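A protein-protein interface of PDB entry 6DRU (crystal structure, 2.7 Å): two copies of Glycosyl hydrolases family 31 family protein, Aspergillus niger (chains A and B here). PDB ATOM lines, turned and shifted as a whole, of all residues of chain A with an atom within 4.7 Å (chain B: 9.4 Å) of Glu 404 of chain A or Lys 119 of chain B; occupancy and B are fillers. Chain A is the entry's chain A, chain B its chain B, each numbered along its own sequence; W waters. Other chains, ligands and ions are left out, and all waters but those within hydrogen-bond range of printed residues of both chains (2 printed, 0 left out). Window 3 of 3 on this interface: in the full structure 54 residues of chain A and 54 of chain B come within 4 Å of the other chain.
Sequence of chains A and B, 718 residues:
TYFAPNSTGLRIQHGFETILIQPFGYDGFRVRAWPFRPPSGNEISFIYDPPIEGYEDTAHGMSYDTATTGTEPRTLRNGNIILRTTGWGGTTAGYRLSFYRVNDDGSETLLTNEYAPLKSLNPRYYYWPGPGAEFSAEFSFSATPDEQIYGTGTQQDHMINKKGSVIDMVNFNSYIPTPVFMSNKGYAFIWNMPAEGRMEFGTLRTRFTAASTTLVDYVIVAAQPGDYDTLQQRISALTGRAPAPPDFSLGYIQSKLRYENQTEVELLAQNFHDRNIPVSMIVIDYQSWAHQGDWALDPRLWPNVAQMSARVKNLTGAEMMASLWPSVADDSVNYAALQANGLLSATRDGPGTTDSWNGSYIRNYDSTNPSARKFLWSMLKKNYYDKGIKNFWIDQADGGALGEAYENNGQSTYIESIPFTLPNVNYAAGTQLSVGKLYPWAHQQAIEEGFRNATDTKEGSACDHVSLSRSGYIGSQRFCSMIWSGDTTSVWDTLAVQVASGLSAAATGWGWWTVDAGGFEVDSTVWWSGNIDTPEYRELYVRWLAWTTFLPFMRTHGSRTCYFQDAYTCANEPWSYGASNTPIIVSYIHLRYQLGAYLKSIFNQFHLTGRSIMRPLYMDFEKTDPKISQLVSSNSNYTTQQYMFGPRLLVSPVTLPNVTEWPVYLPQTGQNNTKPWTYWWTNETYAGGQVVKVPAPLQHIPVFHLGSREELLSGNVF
OE1 of Glu 404 of chain A lies within salt-bridge range of NZ of Lys 119 of chain B, at 3.0 Å. The side-chain hydroxyl (OH) of Tyr 125 of chain B lies within hydrogen-bond range of the backbone NH (N) of Leu 422 of chain A (3.1 Å).
Glu 404 of chain A touches one residue of chain B. Lys 119 of chain B touches four residues of chain A. Of chain B, only Lys 119 comes within 4 Å of Asn 173 of chain A. No residue of chain B comes within 4 Å of Gly 403 of chain A. Of chain B, only Ser 120 (3.2 Å) and Leu 121 (3.9 Å) come within 4 Å of Ala 405 of chain A. Tyr 406 of chain A touches just one residue of chain B: Trp 88 (3.5 Å). Printed residues of chain B within 4 Å of Ser 174 of chain A: Lys 119. Of the printed residues of chain B, Phe 172 of chain A touches Lys 119, Ser 120 and Leu 121. Printed residues of chain A within 4 Å of Trp 88 of chain B: Tyr 406. Pro 117 of chain B touches none of the printed residues of chain A. The nearest residue of chain B that does not touch Glu 404 of chain A is Leu 118 of chain B (5.8 Å). The nearest residue of chain A that does not touch Lys 119 of chain B is Glu 521 of chain A (4.02 Å). The nearest printed residue of chain A that does not touch Ser 120 of chain B is Tyr 406 of chain A (5.3 Å).
Water W1 lies within hydrogen-bond range of the side-chain carboxylate of Glu 521 of chain A (2.5 Å), the side-chain carboxylate of Asp 487 of chain A (2.5 Å) and the side-chain amino group of Lys 119 of chain B (2.6 Å). Water W2 lies within hydrogen-bond range of the backbone NH of Asn 122 of chain B (2.8 Å) and the backbone carbonyl oxygen of Ala 405 of chain A (2.9 Å).
Of the 14 printed residues of chain A, 8 touch a printed residue of chain B. Printed residues of chain A that touch a printed residue of chain B: Phe 172, Asn 173, Ser 174, Glu 404, Ala 405, Tyr 406, Leu 422 and Glu 521. Hydrophobic or aromatic side chains of chain B that line the printed part of chain A: Trp 88, Leu 118, Leu 121 and Tyr 125. Among the printed residues, 12 pairs touch across the chains. Among the printed residues, Asp or Glu carboxylates within 4 Å of a Lys or Arg side-chain nitrogen of the other chain: Glu 404 of chain A with Lys 119 of chain B.
N of Asn 173 of chain A sits at hydrogen-bond distance from O of Gly 403 of chain A (2.9 Å). The side-chain carboxylate (OE2) of Glu 404 of chain A lies within hydrogen-bond range of the side-chain amide nitrogen (ND2) of Asn 173 of chain A. The side-chain amide nitrogen of Asn 173 of chain A sits at hydrogen-bond distance from the side-chain carboxylate of Asp 487 of chain A (2.9 Å). O of Pro 117 of chain B lies within hydrogen-bond range of NE1 of Trp 88 of chain B (3.4 Å). The backbone carbonyl oxygen (O) of Leu 118 of chain B lies within hydrogen-bond range of the indole nitrogen (NE1) of Trp 88 of chain B (3.3 Å). The side-chain hydroxyl of Ser 120 of chain B sits at hydrogen-bond distance from the backbone carbonyl oxygen of Pro 117 of chain B (3.1 Å).
Among the printed residues, merely in contact across the chains: Ala 405 of chain A with Ser 120 of chain B (3.2 Å), Asn 173 of chain A with Lys 119 of chain B (3.4 Å), Glu 521 of chain A with Leu 118 of chain B (3.5 Å), Tyr 406 of chain A with Trp 88 of chain B (3.5 Å), Phe 172 of chain A with Lys 119 of chain B (3.6 Å), Phe 172 of chain A with Ser 120 of chain B (3.7 Å), Leu 422 of chain A with Leu 121 of chain B (3.8 Å), Ser 174 of chain A with Lys 119 of chain B (3.8 Å), Ala 405 of chain A with Leu 121 of chain B (3.9 Å) and Phe 172 of chain A with Leu 121 of chain B (3.99 Å).
No position is printed for both chains.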
ATOM      1  N   PHE A 172      29.631 -10.940 -33.044  1.00  0.00           N
ATOM      2  CA  PHE A 172      29.123 -10.872 -31.678  1.00  0.00           C
ATOM      3  C   PHE A 172      30.111 -10.062 -30.846  1.00  0.00           C
ATOM      4  O   PHE A 172      31.141  -9.603 -31.346  1.00  0.00           O
ATOM      5  CB  PHE A 172      28.863 -12.265 -31.088  1.00  0.00           C
ATOM      6  CG  PHE A 172      30.053 -13.184 -31.112  1.00  0.00           C
ATOM      7  CD1 PHE A 172      31.010 -13.134 -30.110  1.00  0.00           C
ATOM      8  CD2 PHE A 172      30.191 -14.126 -32.119  1.00  0.00           C
ATOM      9  CE1 PHE A 172      32.093 -13.992 -30.124  1.00  0.00           C
ATOM     10  CE2 PHE A 172      31.273 -14.986 -32.140  1.00  0.00           C
ATOM     11  CZ  PHE A 172      32.226 -14.918 -31.142  1.00  0.00           C
ATOM     12  N   ASN A 173      29.771  -9.875 -29.570  1.00  0.00           N
ATOM     13  CA  ASN A 173      30.520  -9.003 -28.667  1.00  0.00           C
ATOM     14  C   ASN A 173      32.010  -9.325 -28.682  1.00  0.00           C
ATOM     15  O   ASN A 173      32.416 -10.448 -28.370  1.00  0.00           O
ATOM     16  CB  ASN A 173      29.960  -9.139 -27.249  1.00  0.00           C
ATOM     17  CG  ASN A 173      30.331  -7.969 -26.354  1.00  0.00           C
ATOM     18  OD1 ASN A 173      31.416  -7.400 -26.474  1.00  0.00           O
ATOM     19  ND2 ASN A 173      29.428  -7.607 -25.451  1.00  0.00           N
ATOM     20  N   SER A 174      32.815  -8.325 -29.059  1.00  0.00           N
ATOM     21  CA  SER A 174      34.284  -8.337 -29.097  1.00  0.00           C
ATOM     22  C   SER A 174      34.845  -9.112 -30.284  1.00  0.00           C
ATOM     23  O   SER A 174      36.066  -9.325 -30.344  1.00  0.00           O
ATOM     24  CB  SER A 174      34.898  -8.902 -27.813  1.00  0.00           C
ATOM     25  OG  SER A 174      34.890 -10.319 -27.834  1.00  0.00           O
ATOM     26  N   GLN A 396      26.172  -2.326 -29.151  1.00  0.00           N
ATOM     27  CA  GLN A 396      25.379  -3.552 -29.272  1.00  0.00           C
ATOM     28  C   GLN A 396      24.698  -3.667 -30.632  1.00  0.00           C
ATOM     29  O   GLN A 396      23.561  -4.132 -30.739  1.00  0.00           O
ATOM     30  CB  GLN A 396      24.352  -3.650 -28.143  1.00  0.00           C
ATOM     31  CG  GLN A 396      24.970  -3.996 -26.811  1.00  0.00           C
ATOM     32  CD  GLN A 396      24.779  -5.449 -26.451  1.00  0.00           C
ATOM     33  OE1 GLN A 396      23.665  -5.965 -26.498  1.00  0.00           O
ATOM     34  NE2 GLN A 396      25.866  -6.121 -26.094  1.00  0.00           N
ATOM     35  N   ALA A 401      21.241 -11.046 -33.692  1.00  0.00           N
ATOM     36  CA  ALA A 401      20.807 -10.976 -32.303  1.00  0.00           C
ATOM     37  C   ALA A 401      21.186  -9.610 -31.732  1.00  0.00           C
ATOM     38  O   ALA A 401      21.617  -8.706 -32.453  1.00  0.00           O
ATOM     39  CB  ALA A 401      21.404 -12.128 -31.500  1.00  0.00           C
ATOM     40  N   LEU A 402      21.041  -9.441 -30.422  1.00  0.00           N
ATOM     41  CA  LEU A 402      21.327  -8.158 -29.784  1.00  0.00           C
ATOM     42  C   LEU A 402      22.721  -8.183 -29.154  1.00  0.00           C
ATOM     43  O   LEU A 402      22.898  -8.155 -27.936  1.00  0.00           O
ATOM     44  CB  LEU A 402      20.246  -7.822 -28.759  1.00  0.00           C
ATOM     45  CG  LEU A 402      20.253  -6.388 -28.222  1.00  0.00           C
ATOM     46  CD1 LEU A 402      20.425  -5.383 -29.352  1.00  0.00           C
ATOM     47  CD2 LEU A 402      18.981  -6.104 -27.440  1.00  0.00           C
ATOM     48  N   GLY A 403      23.727  -8.265 -30.027  1.00  0.00           N
ATOM     49  CA  GLY A 403      25.098  -8.003 -29.644  1.00  0.00           C
ATOM     50  C   GLY A 403      25.882  -9.180 -29.099  1.00  0.00           C
ATOM     51  O   GLY A 403      27.102  -9.056 -28.925  1.00  0.00           O
ATOM     52  N   GLU A 404      25.239 -10.309 -28.819  1.00  0.00           N
ATOM     53  CA  GLU A 404      25.914 -11.453 -28.229  1.00  0.00           C
ATOM     54  C   GLU A 404      25.808 -12.669 -29.139  1.00  0.00           C
ATOM     55  O   GLU A 404      24.998 -12.713 -30.070  1.00  0.00           O
ATOM     56  CB  GLU A 404      25.340 -11.787 -26.846  1.00  0.00           C
ATOM     57  CG  GLU A 404      25.322 -10.615 -25.881  1.00  0.00           C
ATOM     58  CD  GLU A 404      26.694 -10.301 -25.318  1.00  0.00           C
ATOM     59  OE1 GLU A 404      27.631 -11.097 -25.545  1.00  0.00           O
ATOM     60  OE2 GLU A 404      26.836  -9.256 -24.650  1.00  0.00           O
ATOM     61  N   ALA A 405      26.645 -13.664 -28.855  1.00  0.00           N
ATOM     62  CA  ALA A 405      26.652 -14.922 -29.590  1.00  0.00           C
ATOM     63  C   ALA A 405      25.597 -15.897 -29.090  1.00  0.00           C
ATOM     64  O   ALA A 405      25.597 -17.060 -29.505  1.00  0.00           O
ATOM     65  CB  ALA A 405      28.036 -15.568 -29.514  1.00  0.00           C
ATOM     66  N   TYR A 406      24.717 -15.452 -28.198  1.00  0.00           N
ATOM     67  CA  TYR A 406      23.619 -16.257 -27.695  1.00  0.00           C
ATOM     68  C   TYR A 406      22.330 -15.455 -27.781  1.00  0.00           C
ATOM     69  O   TYR A 406      22.344 -14.221 -27.749  1.00  0.00           O
ATOM     70  CB  TYR A 406      23.867 -16.705 -26.247  1.00  0.00           C
ATOM     71  CG  TYR A 406      24.388 -15.605 -25.347  1.00  0.00           C
ATOM     72  CD1 TYR A 406      23.520 -14.720 -24.721  1.00  0.00           C
ATOM     73  CD2 TYR A 406      25.751 -15.451 -25.123  1.00  0.00           C
ATOM     74  CE1 TYR A 406      23.995 -13.713 -23.899  1.00  0.00           C
ATOM     75  CE2 TYR A 406      26.235 -14.448 -24.304  1.00  0.00           C
ATOM     76  CZ  TYR A 406      25.353 -13.583 -23.695  1.00  0.00           C
ATOM     77  OH  TYR A 406      25.831 -12.585 -22.878  1.00  0.00           O
ATOM     78  N   ASN A 409      19.046 -12.488 -24.734  1.00  0.00           N
ATOM     79  CA  ASN A 409      19.908 -11.633 -23.933  1.00  0.00           C
ATOM     80  C   ASN A 409      19.137 -11.045 -22.756  1.00  0.00           C
ATOM     81  O   ASN A 409      17.919 -10.851 -22.813  1.00  0.00           O
ATOM     82  CB  ASN A 409      20.491 -10.516 -24.800  1.00  0.00           C
ATOM     83  CG  ASN A 409      21.654  -9.807 -24.137  1.00  0.00           C
ATOM     84  OD1 ASN A 409      22.143 -10.235 -23.092  1.00  0.00           O
ATOM     85  ND2 ASN A 409      22.106  -8.714 -24.744  1.00  0.00           N
ATOM     86  N   LEU A 422      20.999 -18.839 -33.820  1.00  0.00           N
ATOM     87  CA  LEU A 422      21.085 -17.420 -34.120  1.00  0.00           C
ATOM     88  C   LEU A 422      20.203 -17.089 -35.324  1.00  0.00           C
ATOM     89  O   LEU A 422      20.113 -17.879 -36.268  1.00  0.00           O
ATOM     90  CB  LEU A 422      22.533 -17.019 -34.387  1.00  0.00           C
ATOM     91  CG  LEU A 422      23.427 -17.063 -33.145  1.00  0.00           C
ATOM     92  CD1 LEU A 422      24.839 -16.592 -33.463  1.00  0.00           C
ATOM     93  CD2 LEU A 422      22.820 -16.236 -32.017  1.00  0.00           C
ATOM     94  N   ASP A 487      33.208  -6.046 -24.464  1.00  0.00           N
ATOM     95  CA  ASP A 487      33.115  -6.438 -23.061  1.00  0.00           C
ATOM     96  C   ASP A 487      34.245  -7.396 -22.700  1.00  0.00           C
ATOM     97  O   ASP A 487      34.313  -8.515 -23.220  1.00  0.00           O
ATOM     98  CB  ASP A 487      31.760  -7.080 -22.783  1.00  0.00           C
ATOM     99  CG  ASP A 487      30.618  -6.095 -22.895  1.00  0.00           C
ATOM    100  OD1 ASP A 487      30.892  -4.890 -23.078  1.00  0.00           O
ATOM    101  OD2 ASP A 487      29.450  -6.524 -22.802  1.00  0.00           O
ATOM    102  N   GLU A 521      33.830  -6.210 -17.392  1.00  0.00           N
ATOM    103  CA  GLU A 521      33.086  -7.101 -16.515  1.00  0.00           C
ATOM    104  C   GLU A 521      33.944  -7.581 -15.353  1.00  0.00           C
ATOM    105  O   GLU A 521      35.167  -7.696 -15.457  1.00  0.00           O
ATOM    106  CB  GLU A 521      32.562  -8.316 -17.284  1.00  0.00           C
ATOM    107  CG  GLU A 521      31.300  -8.069 -18.085  1.00  0.00           C
ATOM    108  CD  GLU A 521      30.718  -9.348 -18.652  1.00  0.00           C
ATOM    109  OE1 GLU A 521      31.122 -10.440 -18.198  1.00  0.00           O
ATOM    110  OE2 GLU A 521      29.858  -9.263 -19.553  1.00  0.00           O
ATOM    111  N   TRP B  88      29.275 -22.013 -17.835  1.00  0.00           N
ATOM    112  CA  TRP B  88      29.880 -21.194 -18.876  1.00  0.00           C
ATOM    113  C   TRP B  88      30.112 -19.796 -18.326  1.00  0.00           C
ATOM    114  O   TRP B  88      29.200 -19.190 -17.755  1.00  0.00           O
ATOM    115  CB  TRP B  88      28.997 -21.146 -20.126  1.00  0.00           C
ATOM    116  CG  TRP B  88      29.065 -19.841 -20.849  1.00  0.00           C
ATOM    117  CD1 TRP B  88      30.122 -19.348 -21.558  1.00  0.00           C
ATOM    118  CD2 TRP B  88      28.029 -18.858 -20.935  1.00  0.00           C
ATOM    119  NE1 TRP B  88      29.807 -18.115 -22.078  1.00  0.00           N
ATOM    120  CE2 TRP B  88      28.527 -17.793 -21.710  1.00  0.00           C
ATOM    121  CE3 TRP B  88      26.729 -18.774 -20.430  1.00  0.00           C
ATOM    122  CZ2 TRP B  88      27.770 -16.659 -21.992  1.00  0.00           C
ATOM    123  CZ3 TRP B  88      25.980 -17.650 -20.711  1.00  0.00           C
ATOM    124  CH2 TRP B  88      26.502 -16.608 -21.485  1.00  0.00           C
ATOM    125  N   GLY B  89      31.328 -19.285 -18.506  1.00  0.00           N
ATOM    126  CA  GLY B  89      31.712 -18.064 -17.827  1.00  0.00           C
ATOM    127  C   GLY B  89      32.036 -18.338 -16.367  1.00  0.00           C
ATOM    128  O   GLY B  89      32.524 -19.409 -16.001  1.00  0.00           O
ATOM    129  N   TYR B 115      34.479 -25.814 -26.287  1.00  0.00           N
ATOM    130  CA  TYR B 115      35.001 -24.474 -26.527  1.00  0.00           C
ATOM    131  C   TYR B 115      33.953 -23.418 -26.207  1.00  0.00           C
ATOM    132  O   TYR B 115      33.128 -23.074 -27.059  1.00  0.00           O
ATOM    133  CB  TYR B 115      35.474 -24.324 -27.974  1.00  0.00           C
ATOM    134  CG  TYR B 115      36.112 -22.983 -28.260  1.00  0.00           C
ATOM    135  CD1 TYR B 115      37.411 -22.711 -27.854  1.00  0.00           C
ATOM    136  CD2 TYR B 115      35.413 -21.986 -28.931  1.00  0.00           C
ATOM    137  CE1 TYR B 115      38.000 -21.487 -28.110  1.00  0.00           C
ATOM    138  CE2 TYR B 115      35.994 -20.758 -29.191  1.00  0.00           C
ATOM    139  CZ  TYR B 115      37.287 -20.516 -28.778  1.00  0.00           C
ATOM    140  OH  TYR B 115      37.873 -19.298 -29.033  1.00  0.00           O
ATOM    141  N   ALA B 116      33.980 -22.896 -24.983  1.00  0.00           N
ATOM    142  CA  ALA B 116      33.022 -21.882 -24.541  1.00  0.00           C
ATOM    143  C   ALA B 116      33.713 -20.858 -23.653  1.00  0.00           C
ATOM    144  O   ALA B 116      33.493 -20.814 -22.437  1.00  0.00           O
ATOM    145  CB  ALA B 116      31.842 -22.534 -23.815  1.00  0.00           C
ATOM    146  N   PRO B 117      34.569 -20.000 -24.235  1.00  0.00           N
ATOM    147  CA  PRO B 117      34.990 -18.797 -23.504  1.00  0.00           C
ATOM    148  C   PRO B 117      33.823 -17.832 -23.357  1.00  0.00           C
ATOM    149  O   PRO B 117      32.735 -18.103 -23.875  1.00  0.00           O
ATOM    150  CB  PRO B 117      36.114 -18.221 -24.375  1.00  0.00           C
ATOM    151  CG  PRO B 117      35.870 -18.776 -25.729  1.00  0.00           C
ATOM    152  CD  PRO B 117      35.268 -20.132 -25.525  1.00  0.00           C
ATOM    153  N   LEU B 118      34.033 -16.708 -22.665  1.00  0.00           N
ATOM    154  CA  LEU B 118      32.925 -15.809 -22.346  1.00  0.00           C
ATOM    155  C   LEU B 118      32.174 -15.378 -23.601  1.00  0.00           C
ATOM    156  O   LEU B 118      30.943 -15.467 -23.665  1.00  0.00           O
ATOM    157  CB  LEU B 118      33.440 -14.585 -21.586  1.00  0.00           C
ATOM    158  CG  LEU B 118      32.349 -13.698 -20.983  1.00  0.00           C
ATOM    159  CD1 LEU B 118      31.566 -14.470 -19.935  1.00  0.00           C
ATOM    160  CD2 LEU B 118      32.934 -12.425 -20.387  1.00  0.00           C
ATOM    161  N   LYS B 119      32.900 -14.910 -24.609  1.00  0.00           N
ATOM    162  CA  LYS B 119      32.315 -14.477 -25.874  1.00  0.00           C
ATOM    163  C   LYS B 119      32.679 -15.507 -26.939  1.00  0.00           C
ATOM    164  O   LYS B 119      33.814 -15.538 -27.421  1.00  0.00           O
ATOM    165  CB  LYS B 119      32.802 -13.082 -26.251  1.00  0.00           C
ATOM    166  CG  LYS B 119      32.689 -12.060 -25.131  1.00  0.00           C
ATOM    167  CD  LYS B 119      31.250 -11.620 -24.931  1.00  0.00           C
ATOM    168  CE  LYS B 119      31.005 -11.135 -23.513  1.00  0.00           C
ATOM    169  NZ  LYS B 119      29.628 -10.591 -23.344  1.00  0.00           N
ATOM    170  N   SER B 120      31.709 -16.345 -27.300  1.00  0.00           N
ATOM    171  CA  SER B 120      31.896 -17.377 -28.311  1.00  0.00           C
ATOM    172  C   SER B 120      30.540 -17.985 -28.640  1.00  0.00           C
ATOM    173  O   SER B 120      29.584 -17.871 -27.867  1.00  0.00           O
ATOM    174  CB  SER B 120      32.866 -18.466 -27.842  1.00  0.00           C
ATOM    175  OG  SER B 120      32.310 -19.220 -26.778  1.00  0.00           O
ATOM    176  N   LEU B 121      30.473 -18.636 -29.798  1.00  0.00           N
ATOM    177  CA  LEU B 121      29.258 -19.329 -30.188  1.00  0.00           C
ATOM    178  C   LEU B 121      29.064 -20.578 -29.333  1.00  0.00           C
ATOM    179  O   LEU B 121      29.985 -21.056 -28.663  1.00  0.00           O
ATOM    180  CB  LEU B 121      29.308 -19.710 -31.668  1.00  0.00           C
ATOM    181  CG  LEU B 121      29.632 -18.586 -32.654  1.00  0.00           C
ATOM    182  CD1 LEU B 121      30.185 -19.153 -33.954  1.00  0.00           C
ATOM    183  CD2 LEU B 121      28.396 -17.743 -32.918  1.00  0.00           C
ATOM    184  N   ASN B 122      27.845 -21.098 -29.356  1.00  0.00           N
ATOM    185  CA  ASN B 122      27.517 -22.250 -28.530  1.00  0.00           C
ATOM    186  C   ASN B 122      28.339 -23.455 -28.979  1.00  0.00           C
ATOM    187  O   ASN B 122      28.357 -23.776 -30.175  1.00  0.00           O
ATOM    188  CB  ASN B 122      26.022 -22.560 -28.619  1.00  0.00           C
ATOM    189  CG  ASN B 122      25.538 -23.436 -27.478  1.00  0.00           C
ATOM    190  OD1 ASN B 122      25.800 -24.638 -27.449  1.00  0.00           O
ATOM    191  ND2 ASN B 122      24.819 -22.836 -26.534  1.00  0.00           N
ATOM    192  N   PRO B 123      29.037 -24.137 -28.065  1.00  0.00           N
ATOM    193  CA  PRO B 123      29.858 -25.288 -28.474  1.00  0.00           C
ATOM    194  C   PRO B 123      29.051 -26.458 -29.012  1.00  0.00           C
ATOM    195  O   PRO B 123      29.644 -27.374 -29.597  1.00  0.00           O
ATOM    196  CB  PRO B 123      30.599 -25.667 -27.185  1.00  0.00           C
ATOM    197  CG  PRO B 123      29.753 -25.127 -26.085  1.00  0.00           C
ATOM    198  CD  PRO B 123      29.132 -23.870 -26.620  1.00  0.00           C
ATOM    199  N   TYR B 125      26.125 -26.312 -31.465  1.00  0.00           N
ATOM    200  CA  TYR B 125      25.309 -25.429 -32.285  1.00  0.00           C
ATOM    201  C   TYR B 125      24.416 -26.253 -33.206  1.00  0.00           C
ATOM    202  O   TYR B 125      24.896 -27.152 -33.904  1.00  0.00           O
ATOM    203  CB  TYR B 125      26.193 -24.489 -33.105  1.00  0.00           C
ATOM    204  CG  TYR B 125      25.462 -23.303 -33.689  1.00  0.00           C
ATOM    205  CD1 TYR B 125      24.865 -23.377 -34.939  1.00  0.00           C
ATOM    206  CD2 TYR B 125      25.375 -22.105 -32.990  1.00  0.00           C
ATOM    207  CE1 TYR B 125      24.196 -22.293 -35.477  1.00  0.00           C
ATOM    208  CE2 TYR B 125      24.707 -21.015 -33.519  1.00  0.00           C
ATOM    209  CZ  TYR B 125      24.120 -21.115 -34.763  1.00  0.00           C
ATOM    210  OH  TYR B 125      23.455 -20.035 -35.297  1.00  0.00           O
ATOM    211  N   ARG B 205      40.782 -24.082 -31.365  1.00  0.00           N
ATOM    212  CA  ARG B 205      39.463 -24.700 -31.400  1.00  0.00           C
ATOM    213  C   ARG B 205      39.451 -25.844 -32.402  1.00  0.00           C
ATOM    214  O   ARG B 205      39.907 -25.687 -33.538  1.00  0.00           O
ATOM    215  CB  ARG B 205      38.393 -23.658 -31.747  1.00  0.00           C
ATOM    216  CG  ARG B 205      36.988 -24.205 -31.926  1.00  0.00           C
ATOM    217  CD  ARG B 205      36.021 -23.069 -32.223  1.00  0.00           C
ATOM    218  NE  ARG B 205      36.301 -22.416 -33.498  1.00  0.00           N
ATOM    219  CZ  ARG B 205      35.510 -22.485 -34.563  1.00  0.00           C
ATOM    220  NH1 ARG B 205      34.382 -23.175 -34.505  1.00  0.00           N
ATOM    221  NH2 ARG B 205      35.844 -21.860 -35.682  1.00  0.00           N
HETATM  222  O   HOH W   1      28.892  -8.709 -21.751  1.00  0.00           O
HETATM  223  O   HOH W   2      25.734 -19.764 -30.657  1.00  0.00           O
